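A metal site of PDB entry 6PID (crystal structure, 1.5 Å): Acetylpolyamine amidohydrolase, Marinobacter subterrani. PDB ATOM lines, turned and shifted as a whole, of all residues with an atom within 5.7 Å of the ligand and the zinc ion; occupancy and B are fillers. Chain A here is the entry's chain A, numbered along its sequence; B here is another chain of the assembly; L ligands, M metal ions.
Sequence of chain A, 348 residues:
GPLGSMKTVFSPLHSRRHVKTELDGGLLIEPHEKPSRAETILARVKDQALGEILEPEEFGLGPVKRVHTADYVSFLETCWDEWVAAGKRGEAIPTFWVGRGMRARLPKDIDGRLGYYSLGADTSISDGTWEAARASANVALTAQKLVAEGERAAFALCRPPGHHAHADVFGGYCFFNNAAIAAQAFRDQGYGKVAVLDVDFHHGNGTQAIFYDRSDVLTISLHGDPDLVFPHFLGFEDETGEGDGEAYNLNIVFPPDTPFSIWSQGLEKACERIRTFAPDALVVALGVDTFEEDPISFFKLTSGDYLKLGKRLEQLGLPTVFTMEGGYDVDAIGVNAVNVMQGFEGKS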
ATOM      1  N   GLU A  22      21.543  20.125 -19.818  1.00  0.00           N
ATOM      2  CA  GLU A  22      21.634  20.452 -18.402  1.00  0.00           C
ATOM      3  C   GLU A  22      22.424  21.737 -18.257  1.00  0.00           C
ATOM      4  O   GLU A  22      23.548  21.827 -18.760  1.00  0.00           O
ATOM      5  CB  GLU A  22      22.312  19.332 -17.587  1.00  0.00           C
ATOM      6  CG  GLU A  22      22.541  19.690 -16.105  1.00  0.00           C
ATOM      7  CD  GLU A  22      23.178  18.556 -15.308  1.00  0.00           C
ATOM      8  OE1 GLU A  22      23.197  17.411 -15.794  1.00  0.00           O
ATOM      9  OE2 GLU A  22      23.683  18.820 -14.184  1.00  0.00           O
ATOM     10  N   LEU A  23      21.840  22.736 -17.607  1.00  0.00           N
ATOM     11  CA  LEU A  23      22.588  23.942 -17.304  1.00  0.00           C
ATOM     12  C   LEU A  23      23.650  23.620 -16.249  1.00  0.00           C
ATOM     13  O   LEU A  23      23.334  23.071 -15.189  1.00  0.00           O
ATOM     14  CB  LEU A  23      21.661  25.048 -16.804  1.00  0.00           C
ATOM     15  CG  LEU A  23      22.351  26.348 -16.362  1.00  0.00           C
ATOM     16  CD1 LEU A  23      23.021  27.074 -17.529  1.00  0.00           C
ATOM     17  CD2 LEU A  23      21.397  27.287 -15.622  1.00  0.00           C
ATOM     18  N   ASP A  24      24.899  23.925 -16.566  1.00  0.00           N
ATOM     19  CA  ASP A  24      26.020  23.642 -15.667  1.00  0.00           C
ATOM     20  C   ASP A  24      27.151  24.603 -15.991  1.00  0.00           C
ATOM     21  O   ASP A  24      27.723  24.551 -17.090  1.00  0.00           O
ATOM     22  CB  ASP A  24      26.452  22.192 -15.802  1.00  0.00           C
ATOM     23  CG  ASP A  24      27.444  21.793 -14.752  1.00  0.00           C
ATOM     24  OD1 ASP A  24      27.067  21.739 -13.570  1.00  0.00           O
ATOM     25  OD2 ASP A  24      28.609  21.537 -15.104  1.00  0.00           O
ATOM     26  N   GLY A  25      27.473  25.486 -15.056  1.00  0.00           N
ATOM     27  CA  GLY A  25      28.612  26.372 -15.223  1.00  0.00           C
ATOM     28  C   GLY A  25      28.477  27.326 -16.379  1.00  0.00           C
ATOM     29  O   GLY A  25      29.459  27.588 -17.098  1.00  0.00           O
ATOM     30  N   ILE A  29      25.099  21.479 -21.040  1.00  0.00           N
ATOM     31  CA  ILE A  29      25.963  20.318 -21.172  1.00  0.00           C
ATOM     32  C   ILE A  29      25.114  19.057 -21.292  1.00  0.00           C
ATOM     33  O   ILE A  29      23.890  19.084 -21.147  1.00  0.00           O
ATOM     34  CB  ILE A  29      26.951  20.207 -19.996  1.00  0.00           C
ATOM     35  CG1 ILE A  29      26.263  19.600 -18.779  1.00  0.00           C
ATOM     36  CG2 ILE A  29      27.515  21.578 -19.636  1.00  0.00           C
ATOM     37  CD1 ILE A  29      27.235  19.209 -17.683  1.00  0.00           C
ATOM     38  N   HIS A  32      23.998  14.618 -16.539  1.00  0.00           N
ATOM     39  CA  HIS A  32      24.623  13.585 -15.730  1.00  0.00           C
ATOM     40  C   HIS A  32      23.665  12.445 -15.430  1.00  0.00           C
ATOM     41  O   HIS A  32      24.066  11.285 -15.389  1.00  0.00           O
ATOM     42  CB  HIS A  32      25.117  14.162 -14.411  1.00  0.00           C
ATOM     43  CG  HIS A  32      26.215  15.173 -14.536  1.00  0.00           C
ATOM     44  ND1 HIS A  32      27.539  14.827 -14.725  1.00  0.00           N
ATOM     45  CD2 HIS A  32      26.192  16.531 -14.475  1.00  0.00           C
ATOM     46  CE1 HIS A  32      28.282  15.918 -14.794  1.00  0.00           C
ATOM     47  NE2 HIS A  32      27.484  16.965 -14.647  1.00  0.00           N
ATOM     48  N   ASP A 122      18.958  23.165 -13.461  1.00  0.00           N
ATOM     49  CA  ASP A 122      19.729  22.076 -14.044  1.00  0.00           C
ATOM     50  C   ASP A 122      18.890  20.830 -14.297  1.00  0.00           C
ATOM     51  O   ASP A 122      19.439  19.785 -14.636  1.00  0.00           O
ATOM     52  CB  ASP A 122      20.927  21.735 -13.159  1.00  0.00           C
ATOM     53  CG  ASP A 122      20.519  21.432 -11.730  1.00  0.00           C
ATOM     54  OD1 ASP A 122      19.324  21.528 -11.421  1.00  0.00           O
ATOM     55  OD2 ASP A 122      21.407  21.096 -10.922  1.00  0.00           O
ATOM     56  N   HIS A 163      15.114  12.571  -3.845  1.00  0.00           N
ATOM     57  CA  HIS A 163      15.266  13.099  -2.493  1.00  0.00           C
ATOM     58  C   HIS A 163      15.362  14.620  -2.421  1.00  0.00           C
ATOM     59  O   HIS A 163      15.261  15.185  -1.320  1.00  0.00           O
ATOM     60  CB  HIS A 163      16.456  12.437  -1.771  1.00  0.00           C
ATOM     61  CG  HIS A 163      17.809  12.761  -2.312  1.00  0.00           C
ATOM     62  ND1 HIS A 163      18.913  12.917  -1.501  1.00  0.00           N
ATOM     63  CD2 HIS A 163      18.266  12.918  -3.583  1.00  0.00           C
ATOM     64  CE1 HIS A 163      19.978  13.180  -2.240  1.00  0.00           C
ATOM     65  NE2 HIS A 163      19.610  13.177  -3.506  1.00  0.00           N
ATOM     66  N   HIS A 164      15.490  15.312  -3.550  1.00  0.00           N
ATOM     67  CA  HIS A 164      15.515  16.764  -3.498  1.00  0.00           C
ATOM     68  C   HIS A 164      14.148  17.404  -3.650  1.00  0.00           C
ATOM     69  O   HIS A 164      14.001  18.591  -3.357  1.00  0.00           O
ATOM     70  CB  HIS A 164      16.447  17.309  -4.585  1.00  0.00           C
ATOM     71  CG  HIS A 164      17.888  16.987  -4.350  1.00  0.00           C
ATOM     72  ND1 HIS A 164      18.508  17.199  -3.138  1.00  0.00           N
ATOM     73  CD2 HIS A 164      18.840  16.487  -5.171  1.00  0.00           C
ATOM     74  CE1 HIS A 164      19.782  16.838  -3.219  1.00  0.00           C
ATOM     75  NE2 HIS A 164      20.005  16.416  -4.448  1.00  0.00           N
ATOM     76  N   GLY A 172      17.388  19.333  -8.648  1.00  0.00           N
ATOM     77  CA  GLY A 172      18.417  18.336  -8.399  1.00  0.00           C
ATOM     78  C   GLY A 172      18.102  16.992  -9.032  1.00  0.00           C
ATOM     79  O   GLY A 172      18.413  15.949  -8.449  1.00  0.00           O
ATOM     80  N   TYR A 173      17.456  17.002 -10.194  1.00  0.00           N
ATOM     81  CA  TYR A 173      17.142  15.852 -11.029  1.00  0.00           C
ATOM     82  C   TYR A 173      15.908  15.121 -10.518  1.00  0.00           C
ATOM     83  O   TYR A 173      15.557  14.084 -11.105  1.00  0.00           O
ATOM     84  CB  TYR A 173      18.315  14.861 -11.143  1.00  0.00           C
ATOM     85  CG  TYR A 173      19.681  15.485 -11.466  1.00  0.00           C
ATOM     86  CD1 TYR A 173      19.800  16.657 -12.184  1.00  0.00           C
ATOM     87  CD2 TYR A 173      20.857  14.856 -11.038  1.00  0.00           C
ATOM     88  CE1 TYR A 173      21.073  17.205 -12.484  1.00  0.00           C
ATOM     89  CE2 TYR A 173      22.093  15.376 -11.316  1.00  0.00           C
ATOM     90  CZ  TYR A 173      22.202  16.538 -12.040  1.00  0.00           C
ATOM     91  OH  TYR A 173      23.475  17.030 -12.291  1.00  0.00           O
ATOM     92  N   CYS A 174      15.232  15.625  -9.471  1.00  0.00           N
ATOM     93  CA  CYS A 174      14.139  14.926  -8.793  1.00  0.00           C
ATOM     94  C   CYS A 174      12.802  15.615  -9.020  1.00  0.00           C
ATOM     95  O   CYS A 174      12.725  16.846  -9.000  1.00  0.00           O
ATOM     96  CB  CYS A 174      14.370  14.858  -7.283  1.00  0.00           C
ATOM     97  SG  CYS A 174      15.943  14.139  -6.826  1.00  0.00           S
ATOM     98  N   ASP A 200      22.997   9.221   0.100  1.00  0.00           N
ATOM     99  CA  ASP A 200      23.422   9.973  -1.080  1.00  0.00           C
ATOM    100  C   ASP A 200      24.397  11.069  -0.665  1.00  0.00           C
ATOM    101  O   ASP A 200      24.309  11.619   0.440  1.00  0.00           O
ATOM    102  CB  ASP A 200      22.196  10.567  -1.784  1.00  0.00           C
ATOM    103  CG  ASP A 200      22.534  11.293  -3.077  1.00  0.00           C
ATOM    104  OD1 ASP A 200      22.999  12.461  -3.006  1.00  0.00           O
ATOM    105  OD2 ASP A 200      22.310  10.715  -4.165  1.00  0.00           O
ATOM    106  N   PHE A 201      25.344  11.390  -1.561  1.00  0.00           N
ATOM    107  CA  PHE A 201      26.319  12.437  -1.281  1.00  0.00           C
ATOM    108  C   PHE A 201      25.682  13.774  -0.933  1.00  0.00           C
ATOM    109  O   PHE A 201      26.291  14.585  -0.211  1.00  0.00           O
ATOM    110  CB  PHE A 201      27.266  12.653  -2.478  1.00  0.00           C
ATOM    111  CG  PHE A 201      28.135  13.893  -2.352  1.00  0.00           C
ATOM    112  CD1 PHE A 201      29.271  13.884  -1.551  1.00  0.00           C
ATOM    113  CD2 PHE A 201      27.777  15.084  -2.993  1.00  0.00           C
ATOM    114  CE1 PHE A 201      30.060  15.003  -1.408  1.00  0.00           C
ATOM    115  CE2 PHE A 201      28.562  16.228  -2.849  1.00  0.00           C
ATOM    116  CZ  PHE A 201      29.706  16.192  -2.070  1.00  0.00           C
ATOM    117  N   HIS A 202      24.498  14.068  -1.473  1.00  0.00           N
ATOM    118  CA  HIS A 202      23.858  15.360  -1.284  1.00  0.00           C
ATOM    119  C   HIS A 202      22.789  15.304  -0.212  1.00  0.00           C
ATOM    120  O   HIS A 202      22.183  14.248   0.046  1.00  0.00           O
ATOM    121  CB  HIS A 202      23.200  15.856  -2.580  1.00  0.00           C
ATOM    122  CG  HIS A 202      24.148  16.017  -3.729  1.00  0.00           C
ATOM    123  ND1 HIS A 202      24.309  15.051  -4.691  1.00  0.00           N
ATOM    124  CD2 HIS A 202      24.989  17.020  -4.050  1.00  0.00           C
ATOM    125  CE1 HIS A 202      25.193  15.469  -5.573  1.00  0.00           C
ATOM    126  NE2 HIS A 202      25.624  16.658  -5.200  1.00  0.00           N
ATOM    127  N   PHE A 230      25.643  21.685  -3.587  1.00  0.00           N
ATOM    128  CA  PHE A 230      24.190  21.619  -3.650  1.00  0.00           C
ATOM    129  C   PHE A 230      23.661  20.718  -2.535  1.00  0.00           C
ATOM    130  O   PHE A 230      24.272  19.676  -2.236  1.00  0.00           O
ATOM    131  CB  PHE A 230      23.799  21.063  -5.025  1.00  0.00           C
ATOM    132  CG  PHE A 230      22.323  20.941  -5.226  1.00  0.00           C
ATOM    133  CD1 PHE A 230      21.593  22.021  -5.706  1.00  0.00           C
ATOM    134  CD2 PHE A 230      21.669  19.745  -4.970  1.00  0.00           C
ATOM    135  CE1 PHE A 230      20.229  21.915  -5.906  1.00  0.00           C
ATOM    136  CE2 PHE A 230      20.299  19.639  -5.157  1.00  0.00           C
ATOM    137  CZ  PHE A 230      19.585  20.720  -5.631  1.00  0.00           C
ATOM    138  N   ASP A 289      26.846   8.454  -5.397  1.00  0.00           N
ATOM    139  CA  ASP A 289      27.719   9.582  -5.717  1.00  0.00           C
ATOM    140  C   ASP A 289      28.660   9.941  -4.568  1.00  0.00           C
ATOM    141  O   ASP A 289      29.385  10.939  -4.669  1.00  0.00           O
ATOM    142  CB  ASP A 289      26.930  10.814  -6.198  1.00  0.00           C
ATOM    143  CG  ASP A 289      25.748  11.193  -5.313  1.00  0.00           C
ATOM    144  OD1 ASP A 289      25.513  10.595  -4.249  1.00  0.00           O
ATOM    145  OD2 ASP A 289      25.047  12.151  -5.732  1.00  0.00           O
ATOM    146  N   ILE A 296      30.659  14.772  -9.830  1.00  0.00           N
ATOM    147  CA  ILE A 296      30.189  16.036  -9.284  1.00  0.00           C
ATOM    148  C   ILE A 296      30.310  16.091  -7.761  1.00  0.00           C
ATOM    149  O   ILE A 296      29.782  17.009  -7.142  1.00  0.00           O
ATOM    150  CB  ILE A 296      28.744  16.324  -9.739  1.00  0.00           C
ATOM    151  CG1 ILE A 296      27.808  15.214  -9.244  1.00  0.00           C
ATOM    152  CG2 ILE A 296      28.695  16.470 -11.260  1.00  0.00           C
ATOM    153  CD1 ILE A 296      26.330  15.434  -9.581  1.00  0.00           C
ATOM    154  N   SER A 297      30.999  15.120  -7.141  1.00  0.00           N
ATOM    155  CA  SER A 297      30.992  14.972  -5.696  1.00  0.00           C
ATOM    156  C   SER A 297      32.413  14.802  -5.179  1.00  0.00           C
ATOM    157  O   SER A 297      33.339  14.512  -5.944  1.00  0.00           O
ATOM    158  CB  SER A 297      30.133  13.785  -5.285  1.00  0.00           C
ATOM    159  OG  SER A 297      28.921  13.756  -6.029  1.00  0.00           O
ATOM    160  N   GLU A 325      18.923   6.912  -5.708  1.00  0.00           N
ATOM    161  CA  GLU A 325      19.051   8.351  -5.899  1.00  0.00           C
ATOM    162  C   GLU A 325      20.186   8.658  -6.866  1.00  0.00           C
ATOM    163  O   GLU A 325      20.141   8.272  -8.039  1.00  0.00           O
ATOM    164  CB  GLU A 325      19.263   9.055  -4.551  1.00  0.00           C
ATOM    165  CG  GLU A 325      18.244   8.688  -3.482  1.00  0.00           C
ATOM    166  CD  GLU A 325      16.843   9.195  -3.767  1.00  0.00           C
ATOM    167  OE1 GLU A 325      16.704  10.129  -4.574  1.00  0.00           O
ATOM    168  OE2 GLU A 325      15.887   8.661  -3.186  1.00  0.00           O
ATOM    169  N   GLY A 326      21.240   9.310  -6.386  1.00  0.00           N
ATOM    170  CA  GLY A 326      22.305   9.771  -7.251  1.00  0.00           C
ATOM    171  C   GLY A 326      23.363   8.707  -7.518  1.00  0.00           C
ATOM    172  O   GLY A 326      23.191   7.522  -7.243  1.00  0.00           O
ATOM    173  N   GLY A 327      24.480   9.162  -8.111  1.00  0.00           N
ATOM    174  CA  GLY A 327      25.568   8.311  -8.551  1.00  0.00           C
ATOM    175  C   GLY A 327      25.809   8.434 -10.049  1.00  0.00           C
ATOM    176  O   GLY A 327      24.961   8.007 -10.838  1.00  0.00           O
ATOM    177  N   TYR A 328      26.950   8.998 -10.461  1.00  0.00           N
ATOM    178  CA  TYR A 328      27.114   9.465 -11.843  1.00  0.00           C
ATOM    179  C   TYR A 328      28.387   8.986 -12.532  1.00  0.00           C
ATOM    180  O   TYR A 328      28.588   9.290 -13.722  1.00  0.00           O
ATOM    181  CB  TYR A 328      27.007  11.000 -11.866  1.00  0.00           C
ATOM    182  CG  TYR A 328      25.727  11.420 -11.170  1.00  0.00           C
ATOM    183  CD1 TYR A 328      24.487  11.249 -11.786  1.00  0.00           C
ATOM    184  CD2 TYR A 328      25.750  11.914  -9.873  1.00  0.00           C
ATOM    185  CE1 TYR A 328      23.318  11.602 -11.151  1.00  0.00           C
ATOM    186  CE2 TYR A 328      24.576  12.257  -9.211  1.00  0.00           C
ATOM    187  CZ  TYR A 328      23.362  12.113  -9.867  1.00  0.00           C
ATOM    188  OH  TYR A 328      22.199  12.458  -9.230  1.00  0.00           O
ATOM    189  N   THR B  95      22.638  28.510 -11.237  1.00  0.00           N
ATOM    190  CA  THR B  95      22.026  27.224 -11.524  1.00  0.00           C
ATOM    191  C   THR B  95      21.011  26.801 -10.474  1.00  0.00           C
ATOM    192  O   THR B  95      20.187  25.933 -10.737  1.00  0.00           O
ATOM    193  CB  THR B  95      23.106  26.137 -11.639  1.00  0.00           C
ATOM    194  OG1 THR B  95      24.215  26.667 -12.388  1.00  0.00           O
ATOM    195  CG2 THR B  95      22.568  24.877 -12.338  1.00  0.00           C
ATOM    196  N   PHE B  96      21.073  27.374  -9.268  1.00  0.00           N
ATOM    197  CA  PHE B  96      20.118  26.998  -8.243  1.00  0.00           C
ATOM    198  C   PHE B  96      20.048  28.129  -7.220  1.00  0.00           C
ATOM    199  O   PHE B  96      20.938  28.977  -7.154  1.00  0.00           O
ATOM    200  CB  PHE B  96      20.485  25.655  -7.590  1.00  0.00           C
ATOM    201  CG  PHE B  96      21.953  25.338  -7.635  1.00  0.00           C
ATOM    202  CD1 PHE B  96      22.430  24.260  -8.381  1.00  0.00           C
ATOM    203  CD2 PHE B  96      22.850  26.103  -6.923  1.00  0.00           C
ATOM    204  CE1 PHE B  96      23.788  23.972  -8.413  1.00  0.00           C
ATOM    205  CE2 PHE B  96      24.203  25.813  -6.942  1.00  0.00           C
ATOM    206  CZ  PHE B  96      24.675  24.755  -7.697  1.00  0.00           C
HETATM  207  C1  LIG L   1      24.387  21.382 -11.875  1.00  0.00           C
HETATM  208  C2  LIG L   1      25.040  20.216 -11.045  1.00  0.00           C
HETATM  209  C3  LIG L   1      24.675  20.304  -9.514  1.00  0.00           C
HETATM  210  C4  LIG L   1      24.488  18.919  -8.806  1.00  0.00           C
HETATM  211  C5  LIG L   1      23.000  18.545  -8.469  1.00  0.00           C
HETATM  212  C6  LIG L   1      22.829  17.438  -7.375  1.00  0.00           C
HETATM  213  C7  LIG L   1      22.127  16.147  -7.898  1.00  0.00           C
HETATM  214  C8  LIG L   1      22.207  14.889  -7.039  1.00  0.00           C
HETATM  215  N1  LIG L   1      24.408  21.141 -13.391  1.00  0.00           N
HETATM  216  N2  LIG L   1      21.409  14.671  -5.943  1.00  0.00           N
HETATM  217  O1  LIG L   1      21.562  13.450  -5.242  1.00  0.00           O
HETATM  218  O2  LIG L   1      23.074  14.013  -7.395  1.00  0.00           O
HETATM  219 ZN    ZN M   1      23.429  13.046  -4.942  1.00  0.00          ZN
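The side-chain carboxylate (OD1) of Asp 24 lies within salt-bridge range of a nitrogen (N1) of the ligand (2.7 Å).
The side-chain hydroxyl (OH) of Tyr 328 lies within hydrogen-bond range of an oxygen (O2) of the ligand.
The side-chain carboxylate of Asp 122 is in salt-bridge range of a nitrogen (N1) of the ligand (3.9 Å).
A nitrogen (N1) of the ligand is in salt-bridge range of the side-chain carboxylate (OE2) of Glu 22 (2.6 Å).
NE2 of His 164 lies within hydrogen-bond range of N2 of the ligand (2.7 Å).
The backbone carbonyl oxygen of Leu 23 sits at hydrogen-bond distance from a nitrogen (N1) of the ligand, 2.8 Å away.
A nitrogen (N2) of the ligand lies within hydrogen-bond range of a ring nitrogen (NE2) of His 163, 3.4 Å away.
The backbone NH (N) of Gly 326 sits at hydrogen-bond distance from the side-chain carboxylate (OD2) of Asp 200, 2.8 Å away.
The side-chain carboxylate of Asp 289 sits at hydrogen-bond distance from the backbone NH of Phe 201 (2.8 Å).
The backbone NH (N) of His 163 is in hydrogen-bond range of the side-chain sulfur (SG) of Cys 174, at 3.5 Å.
The backbone NH (N) of His 163 lies within hydrogen-bond range of the side-chain carboxylate (OE1) of Glu 325 (3.0 Å).
The side-chain sulfur (SG) of Cys 174 sits at hydrogen-bond distance from the backbone carbonyl oxygen (O) of Gly 172 (3.5 Å).
OH of Tyr 173 lies within hydrogen-bond range of OE2 of Glu 22, 2.6 Å away.
The side-chain carboxylate (OE1) of Glu 22 is in hydrogen-bond range of the backbone NH (N) of His 32.
NE2 of His 163 is in hydrogen-bond range of NE2 of His 164 (3.4 Å).
O of Gly 172 touches C7 of the ligand, 3.8 Å away.
CE2 of Tyr 173 touches C7 of the ligand, 3.5 Å away.
CD2 of Phe 230 touches C6 of the ligand (3.5 Å).
CG2 of Thr 95 of chain B touches C1 of the ligand (3.97 Å).
CE1 of Phe 96 of chain B touches C3 of the ligand, at 3.9 Å.
15 residues have an atom within 4 Å of the ligand: Glu 22, Leu 23, Asp 24, Asp 122, His 163, His 164, Gly 172, Tyr 173, Asp 200, His 202, Phe 230, Asp 289, Tyr 328, Thr 95 of chain B and Phe 96 of chain B.
Three residues have an atom within 4 Å of the zinc ion: Asp 200, His 202 and Asp 289.
The nearest printed residue that does not touch the zinc ion is His 163 (4.1 Å).
The zinc ion is bound by an oxygen (O1) of the ligand (1.9 Å), the side-chain carboxylate (OD2) of Asp 289 (2.0 Å), the side-chain carboxylate (OD1) of Asp 200 (2.1 Å) and a ring nitrogen (ND1) of His 202 (2.2 Å).
The zinc ion has four donor atoms within binding distance.
Slightly farther from the zinc ion lies O2 of the ligand (2.7 Å).
Slightly farther from the zinc ion lies OD2 of Asp 200 (2.7 Å).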
